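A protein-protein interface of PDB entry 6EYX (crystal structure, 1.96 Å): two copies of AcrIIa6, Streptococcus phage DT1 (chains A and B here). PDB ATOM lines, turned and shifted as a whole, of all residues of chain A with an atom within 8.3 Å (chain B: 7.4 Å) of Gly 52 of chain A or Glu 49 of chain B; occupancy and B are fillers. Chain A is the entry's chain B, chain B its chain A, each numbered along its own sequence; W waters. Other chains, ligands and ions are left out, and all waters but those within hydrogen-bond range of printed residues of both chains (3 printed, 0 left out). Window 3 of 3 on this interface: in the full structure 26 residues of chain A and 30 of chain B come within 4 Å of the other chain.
Among the printed residues, merely in contact across the chains: Ile 3 of chain A with Asn 57 of chain B (3.5 Å), Asn 57 of chain A with Ile 3 of chain B (3.5 Å), Val 56 of chain A with Ala 53 of chain B (3.6 Å), Met 51 of chain A with Gly 52 of chain B (3.6 Å), Gly 52 of chain A with Met 51 of chain B (3.7 Å), Ala 53 of chain A with Ile 48 of chain B (3.7 Å), Ile 48 of chain A with Ala 53 of chain B (3.7 Å), Glu 49 of chain A with Gly 52 of chain B (3.7 Å), Ala 53 of chain A with Val 56 of chain B (3.7 Å), Gly 52 of chain A with Glu 49 of chain B (3.8 Å), Ala 53 of chain A with Ala 53 of chain B (3.8 Å), Ile 3 of chain A with Ala 53 of chain B (3.8 Å), Ile 3 of chain A with Ala 54 of chain B (3.8 Å), Met 51 of chain A with Met 51 of chain B (3.8 Å), Ala 53 of chain A with Ile 3 of chain B (3.9 Å) and Ala 54 of chain A with Ile 3 of chain B (3.9 Å).
Printed residues of chain A that touch a printed residue of chain B: Ile 3, Ile 48, Glu 49, Met 51, Gly 52, Ala 53, Ala 54, Val 56 and Asn 57. Hydrophobic or aromatic side chains of chain A within 4 Å of the printed part of chain B: Ile 3, Ala 53, Ala 54 and Val 56.
Of chain B, only Glu 49 (3.8 Å) and Met 51 (3.7 Å) come within 4 Å of Gly 52 of chain A. Glu 49 of chain B touches three residues of chain A. Of the printed residues of chain A, Ala 53 of chain B touches Ile 3, Ile 48, Glu 49, Met 51, Ala 53 and Val 56. Of the printed residues of chain A, Ala 54 of chain B touches Ile 3 and Glu 49. Printed residues of chain B within 4 Å of Glu 49 of chain A: Gly 52, Ala 53 and Ala 54. Of the printed residues of chain B, Ile 3 of chain A touches Ala 53 (3.8 Å), Ala 54 (3.8 Å) and Asn 57 (3.5 Å). Asp 47 of chain B touches none of the printed residues of chain A. The nearest residue of chain B that does not touch Gly 52 of chain A is Lys 50 of chain B (4.2 Å).
Glu 49 of chain A touches Ala 53 of chain B, and with the chains exchanged Ala 53 of chain A touches Glu 49 of chain B. Met 51 of chain A touches Ala 53 of chain B, and with the chains exchanged Ala 53 of chain A touches Met 51 of chain B. Ala 53 of chain A touches its own counterpart, Ala 53 of chain B. Asn 57 of chain A touches its own counterpart, Asn 57 of chain B. Positions printed for both chains: 3, 46, 47, 48, 49, 50, 51, 52, 53, 54, 56 and 57. Of the 23 pairs that touch across the chains among the printed residues, 23 have their exchanged pair printed and touching as well.
ND2 of Asn 57 of chain A is in hydrogen-bond range of O of Ala 53 of chain A. The backbone carbonyl oxygen (O) of Ala 53 of chain B sits close to the side-chain amide oxygen (OD1) of Asn 57 of chain B. The side-chain carboxylate of Asp 47 of chain B sits close to the backbone NH of Glu 49 of chain B (3.2 Å). The side-chain carboxylate of Asp 47 of chain A lies close to the backbone NH of Glu 49 of chain A (3.2 Å).
O of Met 51 of chain A lies within hydrogen-bond range of N of Ala 53 of chain B (2.9 Å). The backbone NH of Ala 53 of chain B sits at hydrogen-bond distance from the backbone carbonyl oxygen of Glu 49 of chain A (3.4 Å). The backbone NH (N) of Ala 54 of chain A lies within hydrogen-bond range of the backbone carbonyl oxygen (O) of Glu 49 of chain B (3.1 Å). The side-chain amide nitrogen (ND2) of Asn 57 of chain A is in hydrogen-bond range of the side-chain amide oxygen (OD1) of Asn 57 of chain B (3.1 Å). The backbone NH of Ala 53 of chain A lies within hydrogen-bond range of the backbone carbonyl oxygen of Glu 49 of chain B (3.4 Å). The backbone carbonyl oxygen of Met 51 of chain B is in hydrogen-bond range of the backbone NH of Ala 53 of chain A. The backbone NH (N) of Ala 54 of chain B sits at hydrogen-bond distance from the backbone carbonyl oxygen (O) of Glu 49 of chain A, at 3.1 Å.
Water W2 lies within hydrogen-bond range of the backbone carbonyl oxygen of Ala 54 of chain B and the backbone NH of Ile 3 of chain A. Water W1 lies within hydrogen-bond range of the backbone carbonyl oxygen of Ala 54 of chain A (2.7 Å) and the backbone NH of Ile 3 of chain B (3.3 Å). Water W3 lies within hydrogen-bond range of the backbone carbonyl oxygen (O) of Glu 49 of chain B (2.7 Å), the backbone NH (N) of Arg 55 of chain A (3.2 Å) and the side-chain amino group (NZ) of Lys 50 of chain B (3.4 Å).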
ATOM      1  N   ILE A   3      24.614  17.867  -7.270  1.00  0.00           N
ATOM      2  CA  ILE A   3      25.882  17.228  -7.635  1.00  0.00           C
ATOM      3  C   ILE A   3      27.032  18.062  -7.054  1.00  0.00           C
ATOM      4  O   ILE A   3      27.164  19.239  -7.387  1.00  0.00           O
ATOM      5  CB  ILE A   3      26.032  16.986  -9.173  1.00  0.00           C
ATOM      6  CG1 ILE A   3      24.921  16.041  -9.722  1.00  0.00           C
ATOM      7  CG2 ILE A   3      27.455  16.512  -9.550  1.00  0.00           C
ATOM      8  CD1 ILE A   3      24.907  14.566  -9.283  1.00  0.00           C
ATOM      9  N   GLY A  30      28.843   3.910 -20.896  1.00  0.00           N
ATOM     10  CA  GLY A  30      28.212   5.122 -20.366  1.00  0.00           C
ATOM     11  C   GLY A  30      29.015   5.792 -19.261  1.00  0.00           C
ATOM     12  O   GLY A  30      28.746   6.953 -18.918  1.00  0.00           O
ATOM     13  N   THR A  46      39.515  15.799 -10.620  1.00  0.00           N
ATOM     14  CA  THR A  46      38.402  16.057 -11.550  1.00  0.00           C
ATOM     15  C   THR A  46      37.156  16.549 -10.834  1.00  0.00           C
ATOM     16  O   THR A  46      36.596  15.848  -9.997  1.00  0.00           O
ATOM     17  CB  THR A  46      38.125  14.841 -12.452  1.00  0.00           C
ATOM     18  OG1 THR A  46      39.369  14.355 -12.978  1.00  0.00           O
ATOM     19  CG2 THR A  46      37.137  15.132 -13.576  1.00  0.00           C
ATOM     20  N   ASP A  47      36.714  17.755 -11.193  1.00  0.00           N
ATOM     21  CA  ASP A  47      35.536  18.374 -10.608  1.00  0.00           C
ATOM     22  C   ASP A  47      34.276  17.691 -11.145  1.00  0.00           C
ATOM     23  O   ASP A  47      33.930  17.866 -12.314  1.00  0.00           O
ATOM     24  CB  ASP A  47      35.535  19.888 -10.912  1.00  0.00           C
ATOM     25  CG  ASP A  47      34.445  20.696 -10.226  1.00  0.00           C
ATOM     26  OD1 ASP A  47      33.690  20.111  -9.417  1.00  0.00           O
ATOM     27  OD2 ASP A  47      34.365  21.915 -10.477  1.00  0.00           O
ATOM     28  N   ILE A  48      33.596  16.909 -10.272  1.00  0.00           N
ATOM     29  CA  ILE A  48      32.353  16.194 -10.606  1.00  0.00           C
ATOM     30  C   ILE A  48      31.238  17.158 -11.084  1.00  0.00           C
ATOM     31  O   ILE A  48      30.420  16.777 -11.921  1.00  0.00           O
ATOM     32  CB  ILE A  48      31.895  15.274  -9.441  1.00  0.00           C
ATOM     33  CG1 ILE A  48      30.796  14.277  -9.904  1.00  0.00           C
ATOM     34  CG2 ILE A  48      31.482  16.081  -8.189  1.00  0.00           C
ATOM     35  CD1 ILE A  48      30.447  13.139  -8.917  1.00  0.00           C
ATOM     36  N   GLU A  49      31.242  18.405 -10.585  1.00  0.00           N
ATOM     37  CA  GLU A  49      30.263  19.431 -10.970  1.00  0.00           C
ATOM     38  C   GLU A  49      30.357  19.771 -12.459  1.00  0.00           C
ATOM     39  O   GLU A  49      29.344  20.069 -13.086  1.00  0.00           O
ATOM     40  CB  GLU A  49      30.465  20.705 -10.125  1.00  0.00           C
ATOM     41  CG  GLU A  49      30.076  20.518  -8.665  1.00  0.00           C
ATOM     42  CD  GLU A  49      30.190  21.745  -7.776  1.00  0.00           C
ATOM     43  OE1 GLU A  49      30.170  22.879  -8.306  1.00  0.00           O
ATOM     44  OE2 GLU A  49      30.285  21.568  -6.539  1.00  0.00           O
ATOM     45  N   LYS A  50      31.583  19.708 -13.023  1.00  0.00           N
ATOM     46  CA  LYS A  50      31.854  20.033 -14.426  1.00  0.00           C
ATOM     47  C   LYS A  50      31.896  18.819 -15.354  1.00  0.00           C
ATOM     48  O   LYS A  50      31.931  18.998 -16.572  1.00  0.00           O
ATOM     49  CB  LYS A  50      33.145  20.872 -14.567  1.00  0.00           C
ATOM     50  CG  LYS A  50      33.034  22.331 -14.129  1.00  0.00           C
ATOM     51  CD  LYS A  50      31.661  22.941 -14.351  1.00  0.00           C
ATOM     52  CE  LYS A  50      31.718  24.431 -14.317  1.00  0.00           C
ATOM     53  NZ  LYS A  50      32.160  24.945 -12.993  1.00  0.00           N
ATOM     54  N   MET A  51      31.868  17.595 -14.801  1.00  0.00           N
ATOM     55  CA  MET A  51      31.854  16.371 -15.614  1.00  0.00           C
ATOM     56  C   MET A  51      30.528  16.245 -16.366  1.00  0.00           C
ATOM     57  O   MET A  51      29.531  16.820 -15.929  1.00  0.00           O
ATOM     58  CB  MET A  51      32.066  15.142 -14.731  1.00  0.00           C
ATOM     59  CG  MET A  51      33.507  14.958 -14.273  1.00  0.00           C
ATOM     60  SD  MET A  51      33.665  13.618 -13.066  1.00  0.00           S
ATOM     61  CE  MET A  51      33.173  12.216 -14.046  1.00  0.00           C
ATOM     62  N   GLY A  52      30.532  15.495 -17.477  1.00  0.00           N
ATOM     63  CA  GLY A  52      29.351  15.272 -18.308  1.00  0.00           C
ATOM     64  C   GLY A  52      28.191  14.717 -17.502  1.00  0.00           C
ATOM     65  O   GLY A  52      28.374  13.771 -16.725  1.00  0.00           O
ATOM     66  N   ALA A  53      27.008  15.336 -17.644  1.00  0.00           N
ATOM     67  CA  ALA A  53      25.789  14.932 -16.918  1.00  0.00           C
ATOM     68  C   ALA A  53      25.399  13.488 -17.159  1.00  0.00           C
ATOM     69  O   ALA A  53      24.997  12.811 -16.216  1.00  0.00           O
ATOM     70  CB  ALA A  53      24.628  15.844 -17.268  1.00  0.00           C
ATOM     71  N   ALA A  54      25.536  13.006 -18.401  1.00  0.00           N
ATOM     72  CA  ALA A  54      25.175  11.625 -18.715  1.00  0.00           C
ATOM     73  C   ALA A  54      26.106  10.628 -18.011  1.00  0.00           C
ATOM     74  O   ALA A  54      25.628   9.633 -17.475  1.00  0.00           O
ATOM     75  CB  ALA A  54      25.150  11.398 -20.219  1.00  0.00           C
ATOM     76  N   ARG A  55      27.416  10.936 -17.938  1.00  0.00           N
ATOM     77  CA  ARG A  55      28.414  10.102 -17.263  1.00  0.00           C
ATOM     78  C   ARG A  55      28.159   9.991 -15.766  1.00  0.00           C
ATOM     79  O   ARG A  55      28.149   8.884 -15.224  1.00  0.00           O
ATOM     80  CB  ARG A  55      29.793  10.700 -17.448  1.00  0.00           C
ATOM     81  CG  ARG A  55      30.533  10.192 -18.634  1.00  0.00           C
ATOM     82  CD  ARG A  55      31.933  10.696 -18.489  1.00  0.00           C
ATOM     83  NE  ARG A  55      32.890   9.609 -18.386  1.00  0.00           N
ATOM     84  CZ  ARG A  55      34.196   9.760 -18.252  1.00  0.00           C
ATOM     85  NH1 ARG A  55      34.698  10.999 -18.164  1.00  0.00           N
ATOM     86  NH2 ARG A  55      35.012   8.744 -18.212  1.00  0.00           N
ATOM     87  N   VAL A  56      27.981  11.142 -15.102  1.00  0.00           N
ATOM     88  CA  VAL A  56      27.735  11.238 -13.665  1.00  0.00           C
ATOM     89  C   VAL A  56      26.466  10.487 -13.304  1.00  0.00           C
ATOM     90  O   VAL A  56      26.482   9.656 -12.390  1.00  0.00           O
ATOM     91  CB  VAL A  56      27.713  12.714 -13.196  1.00  0.00           C
ATOM     92  CG1 VAL A  56      27.252  12.834 -11.736  1.00  0.00           C
ATOM     93  CG2 VAL A  56      29.080  13.349 -13.368  1.00  0.00           C
ATOM     94  N   ASN A  57      25.376  10.730 -14.057  1.00  0.00           N
ATOM     95  CA  ASN A  57      24.107  10.069 -13.798  1.00  0.00           C
ATOM     96  C   ASN A  57      24.153   8.571 -14.138  1.00  0.00           C
ATOM     97  O   ASN A  57      23.419   7.814 -13.507  1.00  0.00           O
ATOM     98  CB  ASN A  57      22.937  10.807 -14.453  1.00  0.00           C
ATOM     99  CG  ASN A  57      22.635  12.109 -13.733  1.00  0.00           C
ATOM    100  OD1 ASN A  57      21.893  12.150 -12.758  1.00  0.00           O
ATOM    101  ND2 ASN A  57      23.303  13.183 -14.095  1.00  0.00           N
ATOM    102  N   ALA A  58      25.046   8.127 -15.052  1.00  0.00           N
ATOM    103  CA  ALA A  58      25.207   6.701 -15.362  1.00  0.00           C
ATOM    104  C   ALA A  58      25.880   5.974 -14.164  1.00  0.00           C
ATOM    105  O   ALA A  58      25.511   4.839 -13.852  1.00  0.00           O
ATOM    106  CB  ALA A  58      26.026   6.510 -16.642  1.00  0.00           C
ATOM    107  N   MET A  59      26.836   6.656 -13.474  1.00  0.00           N
ATOM    108  CA  MET A  59      27.519   6.114 -12.287  1.00  0.00           C
ATOM    109  C   MET A  59      26.469   5.954 -11.183  1.00  0.00           C
ATOM    110  O   MET A  59      26.392   4.897 -10.558  1.00  0.00           O
ATOM    111  CB  MET A  59      28.639   7.049 -11.809  1.00  0.00           C
ATOM    112  CG  MET A  59      29.888   7.013 -12.704  1.00  0.00           C
ATOM    113  SD  MET A  59      31.339   7.822 -11.966  1.00  0.00           S
ATOM    114  CE  MET A  59      30.948   9.537 -12.186  1.00  0.00           C
ATOM    115  N   LYS B   2      18.423   8.176 -16.799  1.00  0.00           N
ATOM    116  CA  LYS B   2      19.368   8.408 -17.887  1.00  0.00           C
ATOM    117  C   LYS B   2      19.173   9.834 -18.379  1.00  0.00           C
ATOM    118  O   LYS B   2      18.038  10.245 -18.642  1.00  0.00           O
ATOM    119  CB  LYS B   2      19.113   7.455 -19.068  1.00  0.00           C
ATOM    120  CG  LYS B   2      19.259   5.972 -18.760  1.00  0.00           C
ATOM    121  CD  LYS B   2      17.905   5.319 -18.529  1.00  0.00           C
ATOM    122  CE  LYS B   2      18.005   3.821 -18.620  1.00  0.00           C
ATOM    123  NZ  LYS B   2      16.662   3.187 -18.685  1.00  0.00           N
ATOM    124  N   ILE B   3      20.268  10.591 -18.478  1.00  0.00           N
ATOM    125  CA  ILE B   3      20.233  11.941 -19.032  1.00  0.00           C
ATOM    126  C   ILE B   3      20.336  11.827 -20.566  1.00  0.00           C
ATOM    127  O   ILE B   3      21.317  11.267 -21.082  1.00  0.00           O
ATOM    128  CB  ILE B   3      21.351  12.845 -18.433  1.00  0.00           C
ATOM    129  CG1 ILE B   3      21.167  13.047 -16.903  1.00  0.00           C
ATOM    130  CG2 ILE B   3      21.462  14.204 -19.180  1.00  0.00           C
ATOM    131  CD1 ILE B   3      19.911  13.896 -16.445  1.00  0.00           C
ATOM    132  N   ASN B   4      19.319  12.336 -21.291  1.00  0.00           N
ATOM    133  CA  ASN B   4      19.226  12.328 -22.765  1.00  0.00           C
ATOM    134  C   ASN B   4      18.256  13.421 -23.218  1.00  0.00           C
ATOM    135  O   ASN B   4      17.719  14.138 -22.368  1.00  0.00           O
ATOM    136  CB  ASN B   4      18.758  10.938 -23.283  1.00  0.00           C
ATOM    137  CG  ASN B   4      17.432  10.451 -22.695  1.00  0.00           C
ATOM    138  OD1 ASN B   4      16.558  11.220 -22.312  1.00  0.00           O
ATOM    139  ND2 ASN B   4      17.260   9.154 -22.615  1.00  0.00           N
ATOM    140  N   ASP B   5      17.975  13.516 -24.536  1.00  0.00           N
ATOM    141  CA  ASP B   5      17.055  14.498 -25.127  1.00  0.00           C
ATOM    142  C   ASP B   5      15.637  14.427 -24.566  1.00  0.00           C
ATOM    143  O   ASP B   5      15.006  15.474 -24.432  1.00  0.00           O
ATOM    144  CB  ASP B   5      17.060  14.415 -26.659  1.00  0.00           C
ATOM    145  CG  ASP B   5      18.364  14.890 -27.284  1.00  0.00           C
ATOM    146  OD1 ASP B   5      19.225  15.429 -26.546  1.00  0.00           O
ATOM    147  OD2 ASP B   5      18.527  14.723 -28.518  1.00  0.00           O
ATOM    148  N   ASP B   6      15.157  13.229 -24.161  1.00  0.00           N
ATOM    149  CA  ASP B   6      13.832  13.117 -23.525  1.00  0.00           C
ATOM    150  C   ASP B   6      13.767  13.927 -22.231  1.00  0.00           C
ATOM    151  O   ASP B   6      12.722  14.506 -21.926  1.00  0.00           O
ATOM    152  CB  ASP B   6      13.468  11.654 -23.228  1.00  0.00           C
ATOM    153  CG  ASP B   6      13.174  10.805 -24.454  1.00  0.00           C
ATOM    154  OD1 ASP B   6      12.696  11.364 -25.470  1.00  0.00           O
ATOM    155  OD2 ASP B   6      13.323   9.572 -24.363  1.00  0.00           O
ATOM    156  N   LYS B   8      15.781  16.612 -21.575  1.00  0.00           N
ATOM    157  CA  LYS B   8      15.858  18.017 -22.006  1.00  0.00           C
ATOM    158  C   LYS B   8      14.444  18.526 -22.356  1.00  0.00           C
ATOM    159  O   LYS B   8      14.058  19.605 -21.923  1.00  0.00           O
ATOM    160  CB  LYS B   8      16.797  18.168 -23.222  1.00  0.00           C
ATOM    161  CG  LYS B   8      17.052  19.623 -23.605  1.00  0.00           C
ATOM    162  CD  LYS B   8      17.651  19.764 -24.995  1.00  0.00           C
ATOM    163  CE  LYS B   8      16.747  20.596 -25.861  1.00  0.00           C
ATOM    164  NZ  LYS B   8      17.101  20.507 -27.297  1.00  0.00           N
ATOM    165  N   THR B  46      22.707  22.675 -27.797  1.00  0.00           N
ATOM    166  CA  THR B  46      23.525  22.154 -26.695  1.00  0.00           C
ATOM    167  C   THR B  46      23.160  20.711 -26.305  1.00  0.00           C
ATOM    168  O   THR B  46      22.026  20.441 -25.893  1.00  0.00           O
ATOM    169  CB  THR B  46      23.449  23.085 -25.471  1.00  0.00           C
ATOM    170  OG1 THR B  46      23.610  24.433 -25.880  1.00  0.00           O
ATOM    171  CG2 THR B  46      24.537  22.764 -24.447  1.00  0.00           C
ATOM    172  N   ASP B  47      24.141  19.800 -26.379  1.00  0.00           N
ATOM    173  CA  ASP B  47      23.936  18.399 -25.992  1.00  0.00           C
ATOM    174  C   ASP B  47      23.870  18.281 -24.466  1.00  0.00           C
ATOM    175  O   ASP B  47      24.891  18.453 -23.785  1.00  0.00           O
ATOM    176  CB  ASP B  47      25.058  17.521 -26.569  1.00  0.00           C
ATOM    177  CG  ASP B  47      24.920  16.016 -26.358  1.00  0.00           C
ATOM    178  OD1 ASP B  47      23.890  15.574 -25.820  1.00  0.00           O
ATOM    179  OD2 ASP B  47      25.852  15.287 -26.758  1.00  0.00           O
ATOM    180  N   ILE B  48      22.666  17.988 -23.920  1.00  0.00           N
ATOM    181  CA  ILE B  48      22.428  17.842 -22.478  1.00  0.00           C
ATOM    182  C   ILE B  48      23.311  16.739 -21.848  1.00  0.00           C
ATOM    183  O   ILE B  48      23.709  16.863 -20.693  1.00  0.00           O
ATOM    184  CB  ILE B  48      20.916  17.657 -22.162  1.00  0.00           C
ATOM    185  CG1 ILE B  48      20.630  17.838 -20.643  1.00  0.00           C
ATOM    186  CG2 ILE B  48      20.360  16.323 -22.723  1.00  0.00           C
ATOM    187  CD1 ILE B  48      19.146  17.916 -20.237  1.00  0.00           C
ATOM    188  N   GLU B  49      23.650  15.697 -22.627  1.00  0.00           N
ATOM    189  CA  GLU B  49      24.503  14.596 -22.177  1.00  0.00           C
ATOM    190  C   GLU B  49      25.903  15.078 -21.799  1.00  0.00           C
ATOM    191  O   GLU B  49      26.505  14.536 -20.863  1.00  0.00           O
ATOM    192  CB  GLU B  49      24.587  13.509 -23.261  1.00  0.00           C
ATOM    193  CG  GLU B  49      23.280  12.754 -23.463  1.00  0.00           C
ATOM    194  CD  GLU B  49      23.303  11.619 -24.469  1.00  0.00           C
ATOM    195  OE1 GLU B  49      24.403  11.098 -24.775  1.00  0.00           O
ATOM    196  OE2 GLU B  49      22.210  11.234 -24.940  1.00  0.00           O
ATOM    197  N   LYS B  50      26.404  16.110 -22.510  1.00  0.00           N
ATOM    198  CA  LYS B  50      27.738  16.679 -22.311  1.00  0.00           C
ATOM    199  C   LYS B  50      27.778  17.917 -21.423  1.00  0.00           C
ATOM    200  O   LYS B  50      28.876  18.369 -21.063  1.00  0.00           O
ATOM    201  CB  LYS B  50      28.422  16.958 -23.660  1.00  0.00           C
ATOM    202  CG  LYS B  50      28.953  15.705 -24.391  1.00  0.00           C
ATOM    203  CD  LYS B  50      29.371  14.519 -23.474  1.00  0.00           C
ATOM    204  CE  LYS B  50      30.862  14.209 -23.342  1.00  0.00           C
ATOM    205  NZ  LYS B  50      31.241  14.000 -21.911  1.00  0.00           N
ATOM    206  N   MET B  51      26.606  18.461 -21.055  1.00  0.00           N
ATOM    207  CA  MET B  51      26.536  19.624 -20.156  1.00  0.00           C
ATOM    208  C   MET B  51      26.993  19.227 -18.744  1.00  0.00           C
ATOM    209  O   MET B  51      26.918  18.046 -18.394  1.00  0.00           O
ATOM    210  CB  MET B  51      25.108  20.161 -20.089  1.00  0.00           C
ATOM    211  CG  MET B  51      24.709  20.954 -21.297  1.00  0.00           C
ATOM    212  SD  MET B  51      22.955  21.437 -21.298  1.00  0.00           S
ATOM    213  CE  MET B  51      22.890  22.467 -19.862  1.00  0.00           C
ATOM    214  N   GLY B  52      27.460  20.211 -17.964  1.00  0.00           N
ATOM    215  CA  GLY B  52      27.917  20.021 -16.588  1.00  0.00           C
ATOM    216  C   GLY B  52      26.857  19.351 -15.734  1.00  0.00           C
ATOM    217  O   GLY B  52      25.693  19.754 -15.769  1.00  0.00           O
ATOM    218  N   ALA B  53      27.243  18.268 -15.032  1.00  0.00           N
ATOM    219  CA  ALA B  53      26.352  17.479 -14.179  1.00  0.00           C
ATOM    220  C   ALA B  53      25.650  18.309 -13.117  1.00  0.00           C
ATOM    221  O   ALA B  53      24.471  18.087 -12.877  1.00  0.00           O
ATOM    222  CB  ALA B  53      27.115  16.344 -13.526  1.00  0.00           C
ATOM    223  N   ALA B  54      26.365  19.252 -12.479  1.00  0.00           N
ATOM    224  CA  ALA B  54      25.770  20.104 -11.446  1.00  0.00           C
ATOM    225  C   ALA B  54      24.670  20.992 -12.019  1.00  0.00           C
ATOM    226  O   ALA B  54      23.625  21.102 -11.409  1.00  0.00           O
ATOM    227  CB  ALA B  54      26.838  20.943 -10.760  1.00  0.00           C
ATOM    228  N   VAL B  56      22.827  20.496 -14.925  1.00  0.00           N
ATOM    229  CA  VAL B  56      21.703  19.653 -15.359  1.00  0.00           C
ATOM    230  C   VAL B  56      20.866  19.208 -14.161  1.00  0.00           C
ATOM    231  O   VAL B  56      19.637  19.301 -14.207  1.00  0.00           O
ATOM    232  CB  VAL B  56      22.141  18.470 -16.256  1.00  0.00           C
ATOM    233  CG1 VAL B  56      20.989  17.479 -16.478  1.00  0.00           C
ATOM    234  CG2 VAL B  56      22.658  18.972 -17.593  1.00  0.00           C
ATOM    235  N   ASN B  57      21.531  18.728 -13.095  1.00  0.00           N
ATOM    236  CA  ASN B  57      20.833  18.271 -11.896  1.00  0.00           C
ATOM    237  C   ASN B  57      20.221  19.420 -11.090  1.00  0.00           C
ATOM    238  O   ASN B  57      19.222  19.197 -10.415  1.00  0.00           O
ATOM    239  CB  ASN B  57      21.719  17.355 -11.052  1.00  0.00           C
ATOM    240  CG  ASN B  57      21.914  16.012 -11.727  1.00  0.00           C
ATOM    241  OD1 ASN B  57      22.845  15.810 -12.503  1.00  0.00           O
ATOM    242  ND2 ASN B  57      20.989  15.091 -11.533  1.00  0.00           N
HETATM  243  O   HOH W   1      23.027   8.940 -17.855  1.00  0.00           O
HETATM  244  O   HOH W   2      23.373  20.131  -8.926  1.00  0.00           O
HETATM  245  O   HOH W   3      28.521  12.770 -20.325  1.00  0.00           O
